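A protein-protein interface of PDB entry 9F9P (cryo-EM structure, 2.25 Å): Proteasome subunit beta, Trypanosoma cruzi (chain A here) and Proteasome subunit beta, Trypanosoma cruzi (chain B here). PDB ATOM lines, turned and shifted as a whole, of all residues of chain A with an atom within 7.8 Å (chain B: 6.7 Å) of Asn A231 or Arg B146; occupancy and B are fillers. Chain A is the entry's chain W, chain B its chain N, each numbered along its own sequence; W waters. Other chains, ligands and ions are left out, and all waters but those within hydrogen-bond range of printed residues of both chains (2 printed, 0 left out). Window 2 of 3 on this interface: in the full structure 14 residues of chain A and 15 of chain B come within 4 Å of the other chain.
NZ of Lys A227 is in hydrogen-bond range of OE1 of Gln B147, at 3.3 Å.
The guanidinium group (NH1) of Arg B146 sits at hydrogen-bond distance from the side-chain amide oxygen (OD1) of Asn A231 (3.2 Å).
The backbone carbonyl oxygen (O) of Lys A227 sits at hydrogen-bond distance from the side-chain amide nitrogen (ND2) of Asn A231 (2.9 Å).
The backbone carbonyl oxygen (O) of Ala A199 is in hydrogen-bond range of the side-chain hydroxyl (OG) of Ser A202 (2.7 Å).
Among the printed residues, pairs that only touch across the chains: Asn A231 with Pro B143, Lys A227 with Pro B143, Ala A199 with Tyr B139, Ala A199 with Pro B143 and Ser A202 with Leu B144.
Of the printed residues of chain B, Ser A202 touches Leu B144.
Of the printed residues of chain B, Lys A227 touches Pro B143 (3.8 Å) and Gln B147 (3.3 Å).
Asn A231 touches two residues of chain B.
Arg B146 touches just one residue of chain A: Asn A231 (3.2 Å).
The nearest residue of chain B that does not touch Asn A231 is Leu B142 (4.9 Å).
The nearest printed residue of chain B that does not touch Lys A227 is Leu B144 (4.6 Å).
Printed residues of chain A that touch a printed residue of chain B: Ala A199, Ser A202, Lys A227 and Asn A231.
Hydrophobic or aromatic side chains of chain B that line the printed part of chain A: Pro B143 and Leu B144.
Among the printed residues, no Asp or Glu carboxylate lies within 4 Å of a Lys or Arg side-chain nitrogen of the other chain.
Water W2 bridges O of Pro B143 and ND2 of Asn A231.
Water W1 bridges the backbone carbonyl oxygen of Asn A231 (2.7 Å) and the guanidinium group of Arg B146 (3.2 Å).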
ATOM      1  N   SER A 195      28.212 -16.253  -3.268  1.00  0.00           N
ATOM      2  CA  SER A 195      27.737 -15.243  -2.328  1.00  0.00           C
ATOM      3  C   SER A 195      27.840 -15.682  -0.853  1.00  0.00           C
ATOM      4  O   SER A 195      27.935 -14.853   0.031  1.00  0.00           O
ATOM      5  CB  SER A 195      26.269 -14.925  -2.674  1.00  0.00           C
ATOM      6  OG  SER A 195      25.417 -15.980  -2.140  1.00  0.00           O
ATOM      7  N   GLY A 196      27.796 -16.979  -0.569  1.00  0.00           N
ATOM      8  CA  GLY A 196      28.102 -17.462   0.775  1.00  0.00           C
ATOM      9  C   GLY A 196      29.588 -17.738   1.042  1.00  0.00           C
ATOM     10  O   GLY A 196      29.907 -18.341   2.052  1.00  0.00           O
ATOM     11  N   ALA A 199      31.252 -16.512   4.618  1.00  0.00           N
ATOM     12  CA  ALA A 199      30.832 -17.305   5.750  1.00  0.00           C
ATOM     13  C   ALA A 199      31.433 -18.706   5.766  1.00  0.00           C
ATOM     14  O   ALA A 199      31.789 -19.221   6.804  1.00  0.00           O
ATOM     15  CB  ALA A 199      29.354 -17.430   5.681  1.00  0.00           C
ATOM     16  N   ALA A 200      31.496 -19.370   4.607  1.00  0.00           N
ATOM     17  CA  ALA A 200      32.013 -20.731   4.540  1.00  0.00           C
ATOM     18  C   ALA A 200      33.505 -20.772   4.816  1.00  0.00           C
ATOM     19  O   ALA A 200      34.035 -21.700   5.417  1.00  0.00           O
ATOM     20  CB  ALA A 200      31.794 -21.228   3.150  1.00  0.00           C
ATOM     21  N   SER A 202      35.030 -18.950   6.807  1.00  0.00           N
ATOM     22  CA  SER A 202      35.305 -18.835   8.233  1.00  0.00           C
ATOM     23  C   SER A 202      35.382 -20.198   8.919  1.00  0.00           C
ATOM     24  O   SER A 202      36.156 -20.368   9.817  1.00  0.00           O
ATOM     25  CB  SER A 202      34.348 -17.870   8.940  1.00  0.00           C
ATOM     26  OG  SER A 202      33.030 -18.429   9.054  1.00  0.00           O
ATOM     27  N   SER A 223      29.970 -28.603   7.320  1.00  0.00           N
ATOM     28  CA  SER A 223      29.857 -27.491   8.243  1.00  0.00           C
ATOM     29  C   SER A 223      30.108 -26.162   7.514  1.00  0.00           C
ATOM     30  O   SER A 223      29.338 -25.221   7.671  1.00  0.00           O
ATOM     31  CB  SER A 223      30.770 -27.755   9.386  1.00  0.00           C
ATOM     32  OG  SER A 223      31.528 -26.605   9.734  1.00  0.00           O
ATOM     33  N   ALA A 224      31.053 -26.085   6.586  1.00  0.00           N
ATOM     34  CA  ALA A 224      31.186 -24.871   5.808  1.00  0.00           C
ATOM     35  C   ALA A 224      29.962 -24.526   4.962  1.00  0.00           C
ATOM     36  O   ALA A 224      29.650 -23.358   4.832  1.00  0.00           O
ATOM     37  CB  ALA A 224      32.395 -24.964   4.920  1.00  0.00           C
ATOM     38  N   ILE A 225      29.295 -25.517   4.331  1.00  0.00           N
ATOM     39  CA  ILE A 225      28.111 -25.232   3.533  1.00  0.00           C
ATOM     40  C   ILE A 225      26.958 -24.799   4.457  1.00  0.00           C
ATOM     41  O   ILE A 225      26.192 -23.917   4.080  1.00  0.00           O
ATOM     42  CB  ILE A 225      27.688 -26.429   2.647  1.00  0.00           C
ATOM     43  CG1 ILE A 225      28.776 -26.949   1.710  1.00  0.00           C
ATOM     44  CG2 ILE A 225      26.441 -26.084   1.820  1.00  0.00           C
ATOM     45  CD1 ILE A 225      29.106 -25.965   0.641  1.00  0.00           C
ATOM     46  N   ARG A 226      26.801 -25.399   5.643  1.00  0.00           N
ATOM     47  CA  ARG A 226      25.751 -24.941   6.556  1.00  0.00           C
ATOM     48  C   ARG A 226      25.930 -23.499   7.029  1.00  0.00           C
ATOM     49  O   ARG A 226      24.930 -22.827   7.192  1.00  0.00           O
ATOM     50  CB  ARG A 226      25.593 -25.776   7.813  1.00  0.00           C
ATOM     51  CG  ARG A 226      24.969 -27.135   7.552  1.00  0.00           C
ATOM     52  CD  ARG A 226      24.660 -27.888   8.840  1.00  0.00           C
ATOM     53  NE  ARG A 226      25.880 -28.196   9.566  1.00  0.00           N
ATOM     54  CZ  ARG A 226      26.501 -29.373   9.526  1.00  0.00           C
ATOM     55  NH1 ARG A 226      27.625 -29.548  10.208  1.00  0.00           N
ATOM     56  NH2 ARG A 226      25.988 -30.364   8.806  1.00  0.00           N
ATOM     57  N   LYS A 227      27.142 -22.974   7.185  1.00  0.00           N
ATOM     58  CA  LYS A 227      27.296 -21.557   7.452  1.00  0.00           C
ATOM     59  C   LYS A 227      26.704 -20.679   6.343  1.00  0.00           C
ATOM     60  O   LYS A 227      26.133 -19.629   6.597  1.00  0.00           O
ATOM     61  CB  LYS A 227      28.750 -21.102   7.490  1.00  0.00           C
ATOM     62  CG  LYS A 227      29.655 -21.750   8.520  1.00  0.00           C
ATOM     63  CD  LYS A 227      29.373 -21.428   9.918  1.00  0.00           C
ATOM     64  CE  LYS A 227      29.877 -22.543  10.824  1.00  0.00           C
ATOM     65  NZ  LYS A 227      28.928 -23.714  10.806  1.00  0.00           N
ATOM     66  N   GLY A 228      26.881 -21.072   5.080  1.00  0.00           N
ATOM     67  CA  GLY A 228      26.227 -20.339   4.016  1.00  0.00           C
ATOM     68  C   GLY A 228      24.716 -20.477   4.062  1.00  0.00           C
ATOM     69  O   GLY A 228      24.001 -19.508   3.899  1.00  0.00           O
ATOM     70  N   ILE A 229      24.234 -21.690   4.277  1.00  0.00           N
ATOM     71  CA  ILE A 229      22.801 -21.933   4.303  1.00  0.00           C
ATOM     72  C   ILE A 229      22.110 -21.056   5.358  1.00  0.00           C
ATOM     73  O   ILE A 229      21.115 -20.415   5.017  1.00  0.00           O
ATOM     74  CB  ILE A 229      22.539 -23.429   4.521  1.00  0.00           C
ATOM     75  CG1 ILE A 229      22.759 -24.208   3.224  1.00  0.00           C
ATOM     76  CG2 ILE A 229      21.159 -23.683   5.060  1.00  0.00           C
ATOM     77  CD1 ILE A 229      22.801 -25.711   3.399  1.00  0.00           C
ATOM     78  N   PHE A 230      22.660 -20.965   6.593  1.00  0.00           N
ATOM     79  CA  PHE A 230      21.984 -20.235   7.668  1.00  0.00           C
ATOM     80  C   PHE A 230      22.277 -18.743   7.689  1.00  0.00           C
ATOM     81  O   PHE A 230      21.501 -18.011   8.262  1.00  0.00           O
ATOM     82  CB  PHE A 230      22.257 -20.845   9.037  1.00  0.00           C
ATOM     83  CG  PHE A 230      21.632 -22.208   9.150  1.00  0.00           C
ATOM     84  CD1 PHE A 230      20.254 -22.369   9.016  1.00  0.00           C
ATOM     85  CD2 PHE A 230      22.402 -23.347   9.295  1.00  0.00           C
ATOM     86  CE1 PHE A 230      19.654 -23.631   9.075  1.00  0.00           C
ATOM     87  CE2 PHE A 230      21.813 -24.613   9.273  1.00  0.00           C
ATOM     88  CZ  PHE A 230      20.443 -24.754   9.191  1.00  0.00           C
ATOM     89  N   ASN A 231      23.309 -18.243   7.020  1.00  0.00           N
ATOM     90  CA  ASN A 231      23.671 -16.855   7.224  1.00  0.00           C
ATOM     91  C   ASN A 231      23.586 -16.011   5.958  1.00  0.00           C
ATOM     92  O   ASN A 231      23.564 -14.792   6.088  1.00  0.00           O
ATOM     93  CB  ASN A 231      25.047 -16.757   7.877  1.00  0.00           C
ATOM     94  CG  ASN A 231      25.100 -17.499   9.200  1.00  0.00           C
ATOM     95  OD1 ASN A 231      24.547 -17.046  10.199  1.00  0.00           O
ATOM     96  ND2 ASN A 231      25.770 -18.628   9.253  1.00  0.00           N
ATOM     97  N   ASP A 232      23.574 -16.628   4.768  1.00  0.00           N
ATOM     98  CA  ASP A 232      23.485 -15.927   3.494  1.00  0.00           C
ATOM     99  C   ASP A 232      22.100 -16.116   2.872  1.00  0.00           C
ATOM    100  O   ASP A 232      21.658 -17.231   2.580  1.00  0.00           O
ATOM    101  CB  ASP A 232      24.535 -16.433   2.492  1.00  0.00           C
ATOM    102  CG  ASP A 232      24.249 -16.083   1.013  1.00  0.00           C
ATOM    103  OD1 ASP A 232      23.913 -14.907   0.705  1.00  0.00           O
ATOM    104  OD2 ASP A 232      24.387 -16.988   0.136  1.00  0.00           O
ATOM    105  N   PRO A 233      21.359 -15.042   2.571  1.00  0.00           N
ATOM    106  CA  PRO A 233      20.012 -15.193   2.029  1.00  0.00           C
ATOM    107  C   PRO A 233      19.892 -15.861   0.667  1.00  0.00           C
ATOM    108  O   PRO A 233      18.857 -16.467   0.390  1.00  0.00           O
ATOM    109  CB  PRO A 233      19.458 -13.776   1.930  1.00  0.00           C
ATOM    110  CG  PRO A 233      20.656 -12.862   2.109  1.00  0.00           C
ATOM    111  CD  PRO A 233      21.701 -13.650   2.876  1.00  0.00           C
ATOM    112  N   TYR A 234      20.947 -15.801  -0.154  1.00  0.00           N
ATOM    113  CA  TYR A 234      20.929 -16.452  -1.453  1.00  0.00           C
ATOM    114  C   TYR A 234      21.357 -17.925  -1.415  1.00  0.00           C
ATOM    115  O   TYR A 234      21.430 -18.526  -2.467  1.00  0.00           O
ATOM    116  CB  TYR A 234      21.749 -15.637  -2.458  1.00  0.00           C
ATOM    117  CG  TYR A 234      21.191 -14.257  -2.650  1.00  0.00           C
ATOM    118  CD1 TYR A 234      20.065 -14.038  -3.414  1.00  0.00           C
ATOM    119  CD2 TYR A 234      21.706 -13.182  -1.944  1.00  0.00           C
ATOM    120  CE1 TYR A 234      19.503 -12.769  -3.525  1.00  0.00           C
ATOM    121  CE2 TYR A 234      21.139 -11.912  -2.010  1.00  0.00           C
ATOM    122  CZ  TYR A 234      20.040 -11.700  -2.818  1.00  0.00           C
ATOM    123  OH  TYR A 234      19.521 -10.423  -2.893  1.00  0.00           O
ATOM    124  N   SER A 235      21.567 -18.553  -0.274  1.00  0.00           N
ATOM    125  CA  SER A 235      21.917 -19.964  -0.207  1.00  0.00           C
ATOM    126  C   SER A 235      20.928 -20.700   0.672  1.00  0.00           C
ATOM    127  O   SER A 235      20.408 -20.115   1.597  1.00  0.00           O
ATOM    128  CB  SER A 235      23.307 -20.186   0.362  1.00  0.00           C
ATOM    129  OG  SER A 235      24.272 -19.440  -0.343  1.00  0.00           O
ATOM    130  N   ASP B 129      20.783  -8.541  20.517  1.00  0.00           N
ATOM    131  CA  ASP B 129      20.883  -9.983  20.313  1.00  0.00           C
ATOM    132  C   ASP B 129      22.021 -10.533  21.151  1.00  0.00           C
ATOM    133  O   ASP B 129      22.728  -9.768  21.769  1.00  0.00           O
ATOM    134  CB  ASP B 129      21.102 -10.332  18.840  1.00  0.00           C
ATOM    135  CG  ASP B 129      20.680 -11.743  18.426  1.00  0.00           C
ATOM    136  OD1 ASP B 129      20.588 -12.650  19.325  1.00  0.00           O
ATOM    137  OD2 ASP B 129      20.350 -11.938  17.221  1.00  0.00           O
ATOM    138  N   CYS B 131      24.623 -12.067  19.828  1.00  0.00           N
ATOM    139  CA  CYS B 131      25.841 -11.630  19.182  1.00  0.00           C
ATOM    140  C   CYS B 131      25.628 -10.541  18.153  1.00  0.00           C
ATOM    141  O   CYS B 131      24.678 -10.586  17.434  1.00  0.00           O
ATOM    142  CB  CYS B 131      26.591 -12.757  18.483  1.00  0.00           C
ATOM    143  SG  CYS B 131      25.583 -13.810  17.409  1.00  0.00           S
ATOM    144  N   ALA B 138      30.592  -8.799  10.431  1.00  0.00           N
ATOM    145  CA  ALA B 138      29.216  -9.220  10.208  1.00  0.00           C
ATOM    146  C   ALA B 138      29.145 -10.414   9.253  1.00  0.00           C
ATOM    147  O   ALA B 138      28.137 -11.121   9.286  1.00  0.00           O
ATOM    148  CB  ALA B 138      28.406  -8.068   9.672  1.00  0.00           C
ATOM    149  N   TYR B 139      30.155 -10.580   8.379  1.00  0.00           N
ATOM    150  CA  TYR B 139      30.166 -11.636   7.373  1.00  0.00           C
ATOM    151  C   TYR B 139      31.039 -12.786   7.837  1.00  0.00           C
ATOM    152  O   TYR B 139      30.715 -13.926   7.577  1.00  0.00           O
ATOM    153  CB  TYR B 139      30.640 -11.081   6.028  1.00  0.00           C
ATOM    154  CG  TYR B 139      29.752  -9.985   5.529  1.00  0.00           C
ATOM    155  CD1 TYR B 139      28.453 -10.263   5.156  1.00  0.00           C
ATOM    156  CD2 TYR B 139      30.142  -8.661   5.583  1.00  0.00           C
ATOM    157  CE1 TYR B 139      27.579  -9.252   4.762  1.00  0.00           C
ATOM    158  CE2 TYR B 139      29.264  -7.634   5.259  1.00  0.00           C
ATOM    159  CZ  TYR B 139      27.974  -7.926   4.837  1.00  0.00           C
ATOM    160  OH  TYR B 139      27.087  -6.927   4.448  1.00  0.00           O
ATOM    161  N   ALA B 141      32.442 -13.176  11.317  1.00  0.00           N
ATOM    162  CA  ALA B 141      32.374 -13.632  12.694  1.00  0.00           C
ATOM    163  C   ALA B 141      30.997 -14.127  13.119  1.00  0.00           C
ATOM    164  O   ALA B 141      30.919 -15.079  13.852  1.00  0.00           O
ATOM    165  CB  ALA B 141      32.811 -12.507  13.605  1.00  0.00           C
ATOM    166  N   LEU B 142      29.922 -13.449  12.756  1.00  0.00           N
ATOM    167  CA  LEU B 142      28.619 -13.891  13.193  1.00  0.00           C
ATOM    168  C   LEU B 142      28.360 -15.367  12.914  1.00  0.00           C
ATOM    169  O   LEU B 142      27.788 -16.033  13.775  1.00  0.00           O
ATOM    170  CB  LEU B 142      27.508 -13.044  12.551  1.00  0.00           C
ATOM    171  CG  LEU B 142      27.379 -11.630  13.094  1.00  0.00           C
ATOM    172  CD1 LEU B 142      26.246 -10.910  12.431  1.00  0.00           C
ATOM    173  CD2 LEU B 142      27.176 -11.627  14.598  1.00  0.00           C
ATOM    174  N   PRO B 143      28.680 -15.936  11.726  1.00  0.00           N
ATOM    175  CA  PRO B 143      28.494 -17.377  11.498  1.00  0.00           C
ATOM    176  C   PRO B 143      29.143 -18.259  12.545  1.00  0.00           C
ATOM    177  O   PRO B 143      28.505 -19.203  12.962  1.00  0.00           O
ATOM    178  CB  PRO B 143      29.143 -17.622  10.129  1.00  0.00           C
ATOM    179  CG  PRO B 143      28.920 -16.281   9.462  1.00  0.00           C
ATOM    180  CD  PRO B 143      29.274 -15.281  10.554  1.00  0.00           C
ATOM    181  N   LEU B 144      30.369 -17.956  12.962  1.00  0.00           N
ATOM    182  CA  LEU B 144      31.017 -18.719  14.030  1.00  0.00           C
ATOM    183  C   LEU B 144      30.359 -18.474  15.383  1.00  0.00           C
ATOM    184  O   LEU B 144      30.164 -19.442  16.105  1.00  0.00           O
ATOM    185  CB  LEU B 144      32.500 -18.386  14.153  1.00  0.00           C
ATOM    186  CG  LEU B 144      33.406 -18.803  13.003  1.00  0.00           C
ATOM    187  CD1 LEU B 144      34.862 -18.371  13.263  1.00  0.00           C
ATOM    188  CD2 LEU B 144      33.340 -20.313  12.796  1.00  0.00           C
ATOM    189  N   LEU B 145      30.026 -17.231  15.755  1.00  0.00           N
ATOM    190  CA  LEU B 145      29.474 -17.019  17.092  1.00  0.00           C
ATOM    191  C   LEU B 145      28.066 -17.632  17.183  1.00  0.00           C
ATOM    192  O   LEU B 145      27.719 -18.210  18.185  1.00  0.00           O
ATOM    193  CB  LEU B 145      29.434 -15.524  17.417  1.00  0.00           C
ATOM    194  CG  LEU B 145      30.771 -14.772  17.473  1.00  0.00           C
ATOM    195  CD1 LEU B 145      30.522 -13.300  17.515  1.00  0.00           C
ATOM    196  CD2 LEU B 145      31.575 -15.125  18.690  1.00  0.00           C
ATOM    197  N   ARG B 146      27.255 -17.532  16.136  1.00  0.00           N
ATOM    198  CA  ARG B 146      25.926 -18.120  16.133  1.00  0.00           C
ATOM    199  C   ARG B 146      25.933 -19.637  16.300  1.00  0.00           C
ATOM    200  O   ARG B 146      25.076 -20.161  17.008  1.00  0.00           O
ATOM    201  CB  ARG B 146      25.151 -17.789  14.864  1.00  0.00           C
ATOM    202  CG  ARG B 146      24.493 -16.428  14.903  1.00  0.00           C
ATOM    203  CD  ARG B 146      24.213 -15.889  13.532  1.00  0.00           C
ATOM    204  NE  ARG B 146      23.567 -14.586  13.611  1.00  0.00           N
ATOM    205  CZ  ARG B 146      23.413 -13.767  12.580  1.00  0.00           C
ATOM    206  NH1 ARG B 146      23.742 -14.134  11.349  1.00  0.00           N
ATOM    207  NH2 ARG B 146      22.962 -12.545  12.790  1.00  0.00           N
ATOM    208  N   GLN B 147      26.922 -20.325  15.723  1.00  0.00           N
ATOM    209  CA  GLN B 147      27.122 -21.743  15.974  1.00  0.00           C
ATOM    210  C   GLN B 147      27.538 -22.027  17.431  1.00  0.00           C
ATOM    211  O   GLN B 147      27.112 -23.025  17.988  1.00  0.00           O
ATOM    212  CB  GLN B 147      28.136 -22.298  14.967  1.00  0.00           C
ATOM    213  CG  GLN B 147      28.495 -23.775  15.203  1.00  0.00           C
ATOM    214  CD  GLN B 147      29.658 -24.266  14.370  1.00  0.00           C
ATOM    215  OE1 GLN B 147      29.572 -25.282  13.677  1.00  0.00           O
ATOM    216  NE2 GLN B 147      30.786 -23.576  14.471  1.00  0.00           N
ATOM    217  N   ALA B 148      28.402 -21.223  18.054  1.00  0.00           N
ATOM    218  CA  ALA B 148      28.755 -21.460  19.459  1.00  0.00           C
ATOM    219  C   ALA B 148      27.572 -21.262  20.400  1.00  0.00           C
ATOM    220  O   ALA B 148      27.460 -22.008  21.355  1.00  0.00           O
ATOM    221  CB  ALA B 148      29.917 -20.595  19.903  1.00  0.00           C
ATOM    222  N   LEU B 149      26.633 -20.365  20.083  1.00  0.00           N
ATOM    223  CA  LEU B 149      25.467 -20.112  20.938  1.00  0.00           C
ATOM    224  C   LEU B 149      24.350 -21.146  20.755  1.00  0.00           C
ATOM    225  O   LEU B 149      23.319 -21.018  21.396  1.00  0.00           O
ATOM    226  CB  LEU B 149      24.932 -18.711  20.640  1.00  0.00           C
ATOM    227  CG  LEU B 149      25.815 -17.557  21.094  1.00  0.00           C
ATOM    228  CD1 LEU B 149      25.455 -16.278  20.350  1.00  0.00           C
ATOM    229  CD2 LEU B 149      25.680 -17.314  22.568  1.00  0.00           C
ATOM    230  N   GLU B 150      24.517 -22.134  19.862  1.00  0.00           N
ATOM    231  CA  GLU B 150      23.529 -23.190  19.633  1.00  0.00           C
ATOM    232  C   GLU B 150      23.505 -24.198  20.786  1.00  0.00           C
ATOM    233  O   GLU B 150      22.438 -24.696  21.110  1.00  0.00           O
ATOM    234  CB  GLU B 150      23.772 -23.946  18.317  1.00  0.00           C
ATOM    235  CG  GLU B 150      23.188 -23.287  17.061  1.00  0.00           C
ATOM    236  CD  GLU B 150      23.574 -23.961  15.739  1.00  0.00           C
ATOM    237  OE1 GLU B 150      23.832 -23.245  14.733  1.00  0.00           O
ATOM    238  OE2 GLU B 150      23.640 -25.210  15.708  1.00  0.00           O
ATOM    239  N   LYS B 151      24.651 -24.498  21.415  1.00  0.00           N
ATOM    240  CA  LYS B 151      24.673 -25.377  22.580  1.00  0.00           C
ATOM    241  C   LYS B 151      23.684 -24.860  23.624  1.00  0.00           C
ATOM    242  O   LYS B 151      23.581 -23.652  23.843  1.00  0.00           O
ATOM    243  CB  LYS B 151      26.056 -25.469  23.241  1.00  0.00           C
ATOM    244  CG  LYS B 151      26.403 -24.324  24.191  1.00  0.00           C
ATOM    245  CD  LYS B 151      27.747 -24.465  24.881  1.00  0.00           C
ATOM    246  CE  LYS B 151      27.720 -25.434  26.044  1.00  0.00           C
ATOM    247  NZ  LYS B 151      29.041 -26.070  26.250  1.00  0.00           N
HETATM  248  O   HOH W   1      23.917 -13.223   8.285  1.00  0.00           O
HETATM  249  O   HOH W   2      26.474 -20.065  11.865  1.00  0.00           O
